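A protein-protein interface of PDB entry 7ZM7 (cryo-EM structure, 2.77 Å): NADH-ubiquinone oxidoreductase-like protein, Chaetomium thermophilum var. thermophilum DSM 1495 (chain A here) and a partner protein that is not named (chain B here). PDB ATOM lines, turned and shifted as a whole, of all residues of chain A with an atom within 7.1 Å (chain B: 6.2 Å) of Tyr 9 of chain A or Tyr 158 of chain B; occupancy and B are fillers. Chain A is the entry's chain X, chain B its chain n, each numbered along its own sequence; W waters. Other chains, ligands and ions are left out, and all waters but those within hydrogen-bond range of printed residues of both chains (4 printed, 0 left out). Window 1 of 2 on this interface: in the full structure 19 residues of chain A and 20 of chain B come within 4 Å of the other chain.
The guanidinium group of Arg 159 of chain B is in hydrogen-bond range of the side-chain hydroxyl of Thr 8 of chain A, at 3.3 Å. The backbone NH of Tyr 9 of chain A lies close to the guanidinium group of Arg 159 of chain B, 3.4 Å away. The backbone carbonyl oxygen (O) of Gly 165 of chain A lies close to a ring nitrogen (ND1) of His 162 of chain B. The guanidinium group (NH1) of Arg 159 of chain B lies within salt-bridge range of the side-chain carboxylate (OD1) of Asp 167 of chain A (3.0 Å). The side-chain amino group (NZ) of Lys 14 of chain A is in hydrogen-bond range of the backbone carbonyl oxygen (O) of Leu 129 of chain B, 3.2 Å away. A ring nitrogen (NE2) of His 162 of chain B sits at hydrogen-bond distance from the backbone NH of Asp 167 of chain A.
Hydrophobic or aromatic side chains of chain B that line the printed part of chain A: Pro 132, Phe 135, Ile 155, Tyr 158, His 162 and Leu 163. Of the 16 printed residues of chain A, 11 touch a printed residue of chain B. Hydrophobic or aromatic side chains of chain A that line the printed part of chain B: Tyr 9 and Pro 12. Among the printed residues, Asp or Glu carboxylates within 4 Å of a Lys or Arg side-chain nitrogen of the other chain: Asp 167 of chain A with Arg 159 of chain B (3.0 Å).
Water W1 lies within hydrogen-bond range of the backbone carbonyl oxygen of Ser 13 of chain A (2.8 Å), the side-chain hydroxyl of Thr 15 of chain A (2.8 Å), the backbone carbonyl oxygen of Tyr 158 of chain B (3.1 Å) and the side-chain hydroxyl of Tyr 9 of chain A (3.4 Å). Water W3 bridges the backbone carbonyl oxygen (O) of Asp 167 of chain A (3.0 Å) and a ring nitrogen (NE2) of His 162 of chain B (3.3 Å). Water W2 lies within hydrogen-bond range of a ring nitrogen (ND1) of His 162 of chain B (3.0 Å) and the side-chain hydroxyl of Thr 15 of chain A (3.5 Å). Water W4 lies within hydrogen-bond range of OE1 of Gln 161 of chain B, O of Thr 15 of chain A and NZ of Lys 14 of chain A.
The side-chain carboxylate of Asp 167 of chain A is in hydrogen-bond range of the backbone NH of Tyr 9 of chain A, 3.2 Å away. The side-chain hydroxyl (OG1) of Thr 8 of chain A sits at hydrogen-bond distance from the side-chain carboxylate (OD1) of Asp 167 of chain A (2.7 Å). The side-chain amide nitrogen of Asn 25 of chain A lies within hydrogen-bond range of the side-chain hydroxyl of Ser 13 of chain A. The side-chain amide nitrogen (ND2) of Asn 25 of chain A sits close to the backbone NH (N) of Gly 165 of chain A, at 3.5 Å. The backbone carbonyl oxygen of Tyr 9 of chain A lies close to the side-chain amide oxygen of Gln 7 of chain A. The side-chain hydroxyl (OH) of Tyr 9 of chain A sits at hydrogen-bond distance from the backbone NH (N) of Ser 13 of chain A, 3.0 Å away.
Among the printed residues, pairs that only touch across the chains: Thr 15 of chain A with Gln 161 of chain B (3.5 Å), Lys 14 of chain A with Pro 132 of chain B (3.5 Å), Tyr 9 of chain A with Tyr 158 of chain B (3.5 Å), Tyr 9 of chain A with Ile 155 of chain B (3.6 Å), Pro 12 of chain A with Pro 132 of chain B (3.6 Å), Gln 10 of chain A with Ile 155 of chain B (3.6 Å), Thr 15 of chain A with His 162 of chain B (3.6 Å), Pro 12 of chain A with Tyr 158 of chain B (3.6 Å), Asp 167 of chain A with Leu 163 of chain B (3.7 Å), Ser 13 of chain A with Pro 132 of chain B (3.7 Å), Pro 12 of chain A with Phe 135 of chain B (3.7 Å), Val 166 of chain A with His 162 of chain B (3.8 Å), Ser 13 of chain A with Tyr 158 of chain B (3.9 Å) and Gln 7 of chain A with Arg 159 of chain B (3.9 Å).
Tyr 9 of chain A touches three residues of chain B. Tyr 158 of chain B touches three residues of chain A. Printed residues of chain B within 4 Å of Lys 14 of chain A: Leu 129 and Pro 132. Printed residues of chain A within 4 Å of Gln 161 of chain B: Thr 15. Of the printed residues of chain A, Pro 132 of chain B touches Pro 12 (3.6 Å), Ser 13 (3.7 Å) and Lys 14 (3.5 Å). Printed residues of chain B within 4 Å of Thr 15 of chain A: Gln 161 and His 162. Of the printed residues of chain B, Thr 8 of chain A touches Arg 159 (3.3 Å). Glu 156 of chain B touches none of the printed residues of chain A. The nearest residue of chain B that does not touch Tyr 9 of chain A is His 162 of chain B (4.1 Å). The nearest residue of chain A that does not touch Tyr 158 of chain B is Thr 15 of chain A (4.8 Å). The nearest printed residue of chain B that does not touch Thr 15 of chain A is Tyr 158 of chain B (4.8 Å).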
ATOM      1  N   THR A   6      -4.331 -21.296   4.995  1.00  0.00           N
ATOM      2  CA  THR A   6      -5.069 -21.426   3.739  1.00  0.00           C
ATOM      3  C   THR A   6      -5.333 -20.089   3.060  1.00  0.00           C
ATOM      4  O   THR A   6      -5.955 -20.069   1.992  1.00  0.00           O
ATOM      5  CB  THR A   6      -6.409 -22.158   3.909  1.00  0.00           C
ATOM      6  OG1 THR A   6      -7.327 -21.321   4.622  1.00  0.00           O
ATOM      7  CG2 THR A   6      -6.216 -23.461   4.669  1.00  0.00           C
ATOM      8  N   GLN A   7      -4.885 -18.973   3.635  1.00  0.00           N
ATOM      9  CA  GLN A   7      -5.055 -17.660   3.013  1.00  0.00           C
ATOM     10  C   GLN A   7      -3.894 -16.784   3.484  1.00  0.00           C
ATOM     11  O   GLN A   7      -3.929 -16.210   4.572  1.00  0.00           O
ATOM     12  CB  GLN A   7      -6.402 -17.045   3.362  1.00  0.00           C
ATOM     13  CG  GLN A   7      -6.742 -15.839   2.516  1.00  0.00           C
ATOM     14  CD  GLN A   7      -6.853 -16.186   1.051  1.00  0.00           C
ATOM     15  OE1 GLN A   7      -5.943 -15.918   0.269  1.00  0.00           O
ATOM     16  NE2 GLN A   7      -7.973 -16.789   0.668  1.00  0.00           N
ATOM     17  N   THR A   8      -2.891 -16.653   2.630  1.00  0.00           N
ATOM     18  CA  THR A   8      -1.689 -15.871   2.994  1.00  0.00           C
ATOM     19  C   THR A   8      -1.869 -14.442   2.485  1.00  0.00           C
ATOM     20  O   THR A   8      -1.417 -13.517   3.174  1.00  0.00           O
ATOM     21  CB  THR A   8      -0.455 -16.672   2.575  1.00  0.00           C
ATOM     22  OG1 THR A   8      -0.635 -17.040   1.208  1.00  0.00           O
ATOM     23  CG2 THR A   8      -0.285 -17.924   3.407  1.00  0.00           C
ATOM     24  N   TYR A   9      -2.508 -14.265   1.329  1.00  0.00           N
ATOM     25  CA  TYR A   9      -2.843 -12.894   0.873  1.00  0.00           C
ATOM     26  C   TYR A   9      -4.310 -12.681   1.242  1.00  0.00           C
ATOM     27  O   TYR A   9      -5.176 -13.147   0.493  1.00  0.00           O
ATOM     28  CB  TYR A   9      -2.582 -12.765  -0.623  1.00  0.00           C
ATOM     29  CG  TYR A   9      -2.422 -11.364  -1.149  1.00  0.00           C
ATOM     30  CD1 TYR A   9      -1.213 -10.698  -1.051  1.00  0.00           C
ATOM     31  CD2 TYR A   9      -3.473 -10.718  -1.775  1.00  0.00           C
ATOM     32  CE1 TYR A   9      -1.058  -9.415  -1.545  1.00  0.00           C
ATOM     33  CE2 TYR A   9      -3.335  -9.437  -2.278  1.00  0.00           C
ATOM     34  CZ  TYR A   9      -2.125  -8.783  -2.159  1.00  0.00           C
ATOM     35  OH  TYR A   9      -1.991  -7.524  -2.657  1.00  0.00           O
ATOM     36  N   GLN A  10      -4.585 -12.009   2.354  1.00  0.00           N
ATOM     37  CA  GLN A  10      -5.977 -11.904   2.850  1.00  0.00           C
ATOM     38  C   GLN A  10      -6.603 -10.551   2.513  1.00  0.00           C
ATOM     39  O   GLN A  10      -7.836 -10.444   2.593  1.00  0.00           O
ATOM     40  CB  GLN A  10      -5.915 -12.114   4.360  1.00  0.00           C
ATOM     41  CG  GLN A  10      -7.232 -12.541   4.986  1.00  0.00           C
ATOM     42  CD  GLN A  10      -7.105 -12.685   6.481  1.00  0.00           C
ATOM     43  OE1 GLN A  10      -6.005 -12.693   7.030  1.00  0.00           O
ATOM     44  NE2 GLN A  10      -8.238 -12.802   7.154  1.00  0.00           N
ATOM     45  N   PHE A  11      -5.795  -9.567   2.117  1.00  0.00           N
ATOM     46  CA  PHE A  11      -6.310  -8.194   1.902  1.00  0.00           C
ATOM     47  C   PHE A  11      -5.759  -7.635   0.595  1.00  0.00           C
ATOM     48  O   PHE A  11      -4.589  -7.891   0.304  1.00  0.00           O
ATOM     49  CB  PHE A  11      -5.831  -7.310   3.056  1.00  0.00           C
ATOM     50  CG  PHE A  11      -6.429  -7.612   4.406  1.00  0.00           C
ATOM     51  CD1 PHE A  11      -7.581  -6.970   4.828  1.00  0.00           C
ATOM     52  CD2 PHE A  11      -5.834  -8.527   5.258  1.00  0.00           C
ATOM     53  CE1 PHE A  11      -8.131  -7.247   6.069  1.00  0.00           C
ATOM     54  CE2 PHE A  11      -6.389  -8.807   6.497  1.00  0.00           C
ATOM     55  CZ  PHE A  11      -7.534  -8.164   6.900  1.00  0.00           C
ATOM     56  N   PRO A  12      -6.522  -6.842  -0.188  1.00  0.00           N
ATOM     57  CA  PRO A  12      -5.962  -6.221  -1.394  1.00  0.00           C
ATOM     58  C   PRO A  12      -4.890  -5.187  -1.022  1.00  0.00           C
ATOM     59  O   PRO A  12      -5.153  -4.341  -0.209  1.00  0.00           O
ATOM     60  CB  PRO A  12      -7.180  -5.572  -2.064  1.00  0.00           C
ATOM     61  CG  PRO A  12      -8.182  -5.388  -0.942  1.00  0.00           C
ATOM     62  CD  PRO A  12      -7.928  -6.519   0.032  1.00  0.00           C
ATOM     63  N   SER A  13      -3.725  -5.251  -1.658  1.00  0.00           N
ATOM     64  CA  SER A  13      -2.616  -4.338  -1.284  1.00  0.00           C
ATOM     65  C   SER A  13      -2.057  -3.694  -2.544  1.00  0.00           C
ATOM     66  O   SER A  13      -2.271  -4.259  -3.618  1.00  0.00           O
ATOM     67  CB  SER A  13      -1.550  -5.057  -0.505  1.00  0.00           C
ATOM     68  OG  SER A  13      -0.816  -4.147   0.298  1.00  0.00           O
ATOM     69  N   LYS A  14      -1.432  -2.530  -2.401  1.00  0.00           N
ATOM     70  CA  LYS A  14      -0.884  -1.817  -3.578  1.00  0.00           C
ATOM     71  C   LYS A  14       0.484  -2.384  -3.942  1.00  0.00           C
ATOM     72  O   LYS A  14       1.343  -2.450  -3.056  1.00  0.00           O
ATOM     73  CB  LYS A  14      -0.764  -0.320  -3.292  1.00  0.00           C
ATOM     74  CG  LYS A  14      -0.078   0.522  -4.357  1.00  0.00           C
ATOM     75  CD  LYS A  14      -0.905   0.722  -5.601  1.00  0.00           C
ATOM     76  CE  LYS A  14      -0.269   1.701  -6.563  1.00  0.00           C
ATOM     77  NZ  LYS A  14      -1.061   1.850  -7.805  1.00  0.00           N
ATOM     78  N   THR A  15       0.665  -2.779  -5.200  1.00  0.00           N
ATOM     79  CA  THR A  15       2.004  -3.203  -5.674  1.00  0.00           C
ATOM     80  C   THR A  15       2.714  -1.953  -6.200  1.00  0.00           C
ATOM     81  O   THR A  15       2.127  -1.250  -7.038  1.00  0.00           O
ATOM     82  CB  THR A  15       1.917  -4.302  -6.742  1.00  0.00           C
ATOM     83  OG1 THR A  15       1.402  -5.486  -6.135  1.00  0.00           O
ATOM     84  CG2 THR A  15       3.247  -4.596  -7.392  1.00  0.00           C
ATOM     85  N   ASN A  25       5.096  -3.708   3.800  1.00  0.00           N
ATOM     86  CA  ASN A  25       4.436  -2.427   3.594  1.00  0.00           C
ATOM     87  C   ASN A  25       4.517  -1.552   4.829  1.00  0.00           C
ATOM     88  O   ASN A  25       4.566  -0.326   4.723  1.00  0.00           O
ATOM     89  CB  ASN A  25       2.953  -2.624   3.284  1.00  0.00           C
ATOM     90  CG  ASN A  25       2.680  -2.691   1.850  1.00  0.00           C
ATOM     91  OD1 ASN A  25       3.288  -1.979   1.095  1.00  0.00           O
ATOM     92  ND2 ASN A  25       1.695  -3.468   1.458  1.00  0.00           N
ATOM     93  N   GLY A 165       1.273  -6.501   3.136  1.00  0.00           N
ATOM     94  CA  GLY A 165       1.465  -6.453   1.677  1.00  0.00           C
ATOM     95  C   GLY A 165       2.161  -7.646   1.076  1.00  0.00           C
ATOM     96  O   GLY A 165       2.294  -7.666  -0.139  1.00  0.00           O
ATOM     97  N   VAL A 166       2.585  -8.605   1.893  1.00  0.00           N
ATOM     98  CA  VAL A 166       3.379  -9.749   1.376  1.00  0.00           C
ATOM     99  C   VAL A 166       2.599 -11.053   1.469  1.00  0.00           C
ATOM    100  O   VAL A 166       1.817 -11.205   2.417  1.00  0.00           O
ATOM    101  CB  VAL A 166       4.720  -9.848   2.110  1.00  0.00           C
ATOM    102  CG1 VAL A 166       5.680  -8.774   1.628  1.00  0.00           C
ATOM    103  CG2 VAL A 166       4.549  -9.777   3.616  1.00  0.00           C
ATOM    104  N   ASP A 167       2.812 -11.949   0.508  1.00  0.00           N
ATOM    105  CA  ASP A 167       2.189 -13.291   0.539  1.00  0.00           C
ATOM    106  C   ASP A 167       3.021 -14.103   1.515  1.00  0.00           C
ATOM    107  O   ASP A 167       4.168 -14.369   1.201  1.00  0.00           O
ATOM    108  CB  ASP A 167       2.168 -13.900  -0.863  1.00  0.00           C
ATOM    109  CG  ASP A 167       1.138 -14.988  -1.042  1.00  0.00           C
ATOM    110  OD1 ASP A 167       0.117 -14.918  -0.358  1.00  0.00           O
ATOM    111  OD2 ASP A 167       1.375 -15.886  -1.862  1.00  0.00           O
ATOM    112  N   THR A 168       2.476 -14.444   2.670  1.00  0.00           N
ATOM    113  CA  THR A 168       3.234 -15.096   3.729  1.00  0.00           C
ATOM    114  C   THR A 168       3.356 -16.599   3.549  1.00  0.00           C
ATOM    115  O   THR A 168       3.754 -17.287   4.488  1.00  0.00           O
ATOM    116  CB  THR A 168       2.625 -14.787   5.100  1.00  0.00           C
ATOM    117  OG1 THR A 168       1.248 -15.167   5.129  1.00  0.00           O
ATOM    118  CG2 THR A 168       2.733 -13.323   5.384  1.00  0.00           C
ATOM    119  N   ALA A 169       3.002 -17.127   2.390  1.00  0.00           N
ATOM    120  CA  ALA A 169       3.176 -18.570   2.126  1.00  0.00           C
ATOM    121  C   ALA A 169       4.648 -18.984   2.268  1.00  0.00           C
ATOM    122  O   ALA A 169       4.884 -20.036   2.851  1.00  0.00           O
ATOM    123  CB  ALA A 169       2.694 -18.842   0.744  1.00  0.00           C
ATOM    124  N   LEU B 129      -5.991   1.874  -9.225  1.00  0.00           N
ATOM    125  CA  LEU B 129      -6.299   2.561  -7.959  1.00  0.00           C
ATOM    126  C   LEU B 129      -4.996   2.802  -7.204  1.00  0.00           C
ATOM    127  O   LEU B 129      -4.224   1.847  -7.064  1.00  0.00           O
ATOM    128  CB  LEU B 129      -7.275   1.682  -7.170  1.00  0.00           C
ATOM    129  CG  LEU B 129      -8.695   1.624  -7.721  1.00  0.00           C
ATOM    130  CD1 LEU B 129      -9.511   0.584  -6.974  1.00  0.00           C
ATOM    131  CD2 LEU B 129      -9.352   2.989  -7.624  1.00  0.00           C
ATOM    132  N   PRO B 132      -5.910   0.703  -3.501  1.00  0.00           N
ATOM    133  CA  PRO B 132      -6.711  -0.533  -3.613  1.00  0.00           C
ATOM    134  C   PRO B 132      -7.213  -1.016  -2.254  1.00  0.00           C
ATOM    135  O   PRO B 132      -7.829  -2.039  -2.212  1.00  0.00           O
ATOM    136  CB  PRO B 132      -5.702  -1.611  -4.034  1.00  0.00           C
ATOM    137  CG  PRO B 132      -4.390  -1.056  -3.606  1.00  0.00           C
ATOM    138  CD  PRO B 132      -4.534   0.405  -3.949  1.00  0.00           C
ATOM    139  N   PHE B 135     -11.081  -1.417  -0.900  1.00  0.00           N
ATOM    140  CA  PHE B 135     -11.950  -2.619  -0.961  1.00  0.00           C
ATOM    141  C   PHE B 135     -12.127  -3.165   0.454  1.00  0.00           C
ATOM    142  O   PHE B 135     -13.076  -3.935   0.675  1.00  0.00           O
ATOM    143  CB  PHE B 135     -11.353  -3.676  -1.882  1.00  0.00           C
ATOM    144  CG  PHE B 135     -11.579  -3.432  -3.352  1.00  0.00           C
ATOM    145  CD1 PHE B 135     -12.813  -3.677  -3.929  1.00  0.00           C
ATOM    146  CD2 PHE B 135     -10.554  -2.973  -4.162  1.00  0.00           C
ATOM    147  CE1 PHE B 135     -13.015  -3.464  -5.281  1.00  0.00           C
ATOM    148  CE2 PHE B 135     -10.759  -2.754  -5.514  1.00  0.00           C
ATOM    149  CZ  PHE B 135     -11.987  -3.004  -6.070  1.00  0.00           C
ATOM    150  N   HIS B 153     -12.627 -12.493  -5.876  1.00  0.00           N
ATOM    151  CA  HIS B 153     -12.135 -12.359  -7.265  1.00  0.00           C
ATOM    152  C   HIS B 153     -11.216 -11.145  -7.304  1.00  0.00           C
ATOM    153  O   HIS B 153     -10.244 -11.155  -8.074  1.00  0.00           O
ATOM    154  CB  HIS B 153     -13.311 -12.288  -8.240  1.00  0.00           C
ATOM    155  CG  HIS B 153     -14.179 -11.082  -8.101  1.00  0.00           C
ATOM    156  ND1 HIS B 153     -14.353 -10.183  -9.130  1.00  0.00           N
ATOM    157  CD2 HIS B 153     -14.934 -10.633  -7.074  1.00  0.00           C
ATOM    158  CE1 HIS B 153     -15.174  -9.230  -8.747  1.00  0.00           C
ATOM    159  NE2 HIS B 153     -15.543  -9.480  -7.488  1.00  0.00           N
ATOM    160  N   VAL B 154     -11.516 -10.139  -6.486  1.00  0.00           N
ATOM    161  CA  VAL B 154     -10.673  -8.957  -6.374  1.00  0.00           C
ATOM    162  C   VAL B 154      -9.365  -9.302  -5.692  1.00  0.00           C
ATOM    163  O   VAL B 154      -8.292  -8.887  -6.139  1.00  0.00           O
ATOM    164  CB  VAL B 154     -11.439  -7.853  -5.632  1.00  0.00           C
ATOM    165  CG1 VAL B 154     -10.582  -6.645  -5.392  1.00  0.00           C
ATOM    166  CG2 VAL B 154     -12.617  -7.462  -6.439  1.00  0.00           C
ATOM    167  N   ILE B 155      -9.428 -10.055  -4.595  1.00  0.00           N
ATOM    168  CA  ILE B 155      -8.217 -10.359  -3.841  1.00  0.00           C
ATOM    169  C   ILE B 155      -7.301 -11.274  -4.637  1.00  0.00           C
ATOM    170  O   ILE B 155      -6.077 -11.134  -4.591  1.00  0.00           O
ATOM    171  CB  ILE B 155      -8.564 -10.949  -2.464  1.00  0.00           C
ATOM    172  CG1 ILE B 155      -9.325  -9.933  -1.624  1.00  0.00           C
ATOM    173  CG2 ILE B 155      -7.321 -11.383  -1.731  1.00  0.00           C
ATOM    174  CD1 ILE B 155      -9.901 -10.510  -0.395  1.00  0.00           C
ATOM    175  N   GLU B 156      -7.879 -12.125  -5.477  1.00  0.00           N
ATOM    176  CA  GLU B 156      -7.024 -12.966  -6.346  1.00  0.00           C
ATOM    177  C   GLU B 156      -6.357 -12.129  -7.442  1.00  0.00           C
ATOM    178  O   GLU B 156      -5.253 -12.498  -7.842  1.00  0.00           O
ATOM    179  CB  GLU B 156      -7.815 -14.134  -6.921  1.00  0.00           C
ATOM    180  CG  GLU B 156      -7.960 -15.279  -5.938  1.00  0.00           C
ATOM    181  CD  GLU B 156      -6.640 -15.844  -5.442  1.00  0.00           C
ATOM    182  OE1 GLU B 156      -5.742 -16.068  -6.279  1.00  0.00           O
ATOM    183  OE2 GLU B 156      -6.509 -16.049  -4.220  1.00  0.00           O
ATOM    184  N   HIS B 157      -6.972 -11.038  -7.883  1.00  0.00           N
ATOM    185  CA  HIS B 157      -6.331 -10.119  -8.855  1.00  0.00           C
ATOM    186  C   HIS B 157      -5.064  -9.574  -8.226  1.00  0.00           C
ATOM    187  O   HIS B 157      -3.995  -9.708  -8.822  1.00  0.00           O
ATOM    188  CB  HIS B 157      -7.342  -9.050  -9.290  1.00  0.00           C
ATOM    189  CG  HIS B 157      -6.799  -7.940 -10.120  1.00  0.00           C
ATOM    190  ND1 HIS B 157      -6.826  -7.973 -11.495  1.00  0.00           N
ATOM    191  CD2 HIS B 157      -6.250  -6.757  -9.776  1.00  0.00           C
ATOM    192  CE1 HIS B 157      -6.297  -6.865 -11.966  1.00  0.00           C
ATOM    193  NE2 HIS B 157      -5.935  -6.104 -10.933  1.00  0.00           N
ATOM    194  N   TYR B 158      -5.219  -8.934  -7.074  1.00  0.00           N
ATOM    195  CA  TYR B 158      -4.095  -8.291  -6.357  1.00  0.00           C
ATOM    196  C   TYR B 158      -3.056  -9.322  -5.927  1.00  0.00           C
ATOM    197  O   TYR B 158      -1.878  -8.964  -5.885  1.00  0.00           O
ATOM    198  CB  TYR B 158      -4.681  -7.379  -5.275  1.00  0.00           C
ATOM    199  CG  TYR B 158      -5.358  -6.149  -5.823  1.00  0.00           C
ATOM    200  CD1 TYR B 158      -4.637  -5.198  -6.522  1.00  0.00           C
ATOM    201  CD2 TYR B 158      -6.715  -5.939  -5.663  1.00  0.00           C
ATOM    202  CE1 TYR B 158      -5.242  -4.067  -7.039  1.00  0.00           C
ATOM    203  CE2 TYR B 158      -7.336  -4.811  -6.171  1.00  0.00           C
ATOM    204  CZ  TYR B 158      -6.596  -3.870  -6.863  1.00  0.00           C
ATOM    205  OH  TYR B 158      -7.187  -2.751  -7.372  1.00  0.00           O
ATOM    206  N   ARG B 159      -3.471 -10.534  -5.564  1.00  0.00           N
ATOM    207  CA  ARG B 159      -2.487 -11.588  -5.226  1.00  0.00           C
ATOM    208  C   ARG B 159      -1.620 -11.880  -6.448  1.00  0.00           C
ATOM    209  O   ARG B 159      -0.397 -11.895  -6.310  1.00  0.00           O
ATOM    210  CB  ARG B 159      -3.200 -12.877  -4.816  1.00  0.00           C
ATOM    211  CG  ARG B 159      -2.273 -13.955  -4.281  1.00  0.00           C
ATOM    212  CD  ARG B 159      -2.999 -15.269  -4.095  1.00  0.00           C
ATOM    213  NE  ARG B 159      -2.091 -16.346  -3.735  1.00  0.00           N
ATOM    214  CZ  ARG B 159      -1.827 -16.729  -2.493  1.00  0.00           C
ATOM    215  NH1 ARG B 159      -2.411 -16.124  -1.472  1.00  0.00           N
ATOM    216  NH2 ARG B 159      -0.982 -17.721  -2.274  1.00  0.00           N
ATOM    217  N   LYS B 160      -2.239 -12.009  -7.614  1.00  0.00           N
ATOM    218  CA  LYS B 160      -1.492 -12.304  -8.856  1.00  0.00           C
ATOM    219  C   LYS B 160      -0.544 -11.147  -9.149  1.00  0.00           C
ATOM    220  O   LYS B 160       0.561 -11.409  -9.616  1.00  0.00           O
ATOM    221  CB  LYS B 160      -2.462 -12.545 -10.012  1.00  0.00           C
ATOM    222  CG  LYS B 160      -1.830 -13.056 -11.299  1.00  0.00           C
ATOM    223  CD  LYS B 160      -2.802 -13.155 -12.452  1.00  0.00           C
ATOM    224  CE  LYS B 160      -2.151 -13.656 -13.723  1.00  0.00           C
ATOM    225  NZ  LYS B 160      -3.128 -13.784 -14.829  1.00  0.00           N
ATOM    226  N   GLN B 161      -0.985  -9.913  -8.924  1.00  0.00           N
ATOM    227  CA  GLN B 161      -0.151  -8.712  -9.202  1.00  0.00           C
ATOM    228  C   GLN B 161       1.091  -8.697  -8.308  1.00  0.00           C
ATOM    229  O   GLN B 161       2.168  -8.367  -8.814  1.00  0.00           O
ATOM    230  CB  GLN B 161      -1.014  -7.459  -9.101  1.00  0.00           C
ATOM    231  CG  GLN B 161      -0.233  -6.157  -9.133  1.00  0.00           C
ATOM    232  CD  GLN B 161      -1.140  -4.957  -9.239  1.00  0.00           C
ATOM    233  OE1 GLN B 161      -0.701  -3.812  -9.181  1.00  0.00           O
ATOM    234  NE2 GLN B 161      -2.426  -5.218  -9.395  1.00  0.00           N
ATOM    235  N   HIS B 162       0.955  -9.078  -7.042  1.00  0.00           N
ATOM    236  CA  HIS B 162       2.090  -9.067  -6.083  1.00  0.00           C
ATOM    237  C   HIS B 162       3.049 -10.203  -6.431  1.00  0.00           C
ATOM    238  O   HIS B 162       4.266 -10.016  -6.299  1.00  0.00           O
ATOM    239  CB  HIS B 162       1.571  -9.231  -4.646  1.00  0.00           C
ATOM    240  CG  HIS B 162       2.637  -9.528  -3.646  1.00  0.00           C
ATOM    241  ND1 HIS B 162       3.388  -8.536  -3.053  1.00  0.00           N
ATOM    242  CD2 HIS B 162       3.093 -10.697  -3.147  1.00  0.00           C
ATOM    243  CE1 HIS B 162       4.262  -9.077  -2.234  1.00  0.00           C
ATOM    244  NE2 HIS B 162       4.099 -10.403  -2.273  1.00  0.00           N
ATOM    245  N   LEU B 163       2.495 -11.352  -6.809  1.00  0.00           N
ATOM    246  CA  LEU B 163       3.329 -12.526  -7.140  1.00  0.00           C
ATOM    247  C   LEU B 163       4.074 -12.292  -8.449  1.00  0.00           C
ATOM    248  O   LEU B 163       5.266 -12.580  -8.484  1.00  0.00           O
ATOM    249  CB  LEU B 163       2.432 -13.761  -7.145  1.00  0.00           C
ATOM    250  CG  LEU B 163       1.880 -14.160  -5.778  1.00  0.00           C
ATOM    251  CD1 LEU B 163       0.942 -15.350  -5.892  1.00  0.00           C
ATOM    252  CD2 LEU B 163       3.005 -14.456  -4.800  1.00  0.00           C
HETATM  253  O   HOH W   1      -1.309  -5.913  -5.594  1.00  0.00           O
HETATM  254  O   HOH W   2       3.064  -5.516  -3.089  1.00  0.00           O
HETATM  255  O   HOH W   3       5.822 -12.507  -0.413  1.00  0.00           O
HETATM  256  O   HOH W   4       0.005  -0.761  -9.431  1.00  0.00           O
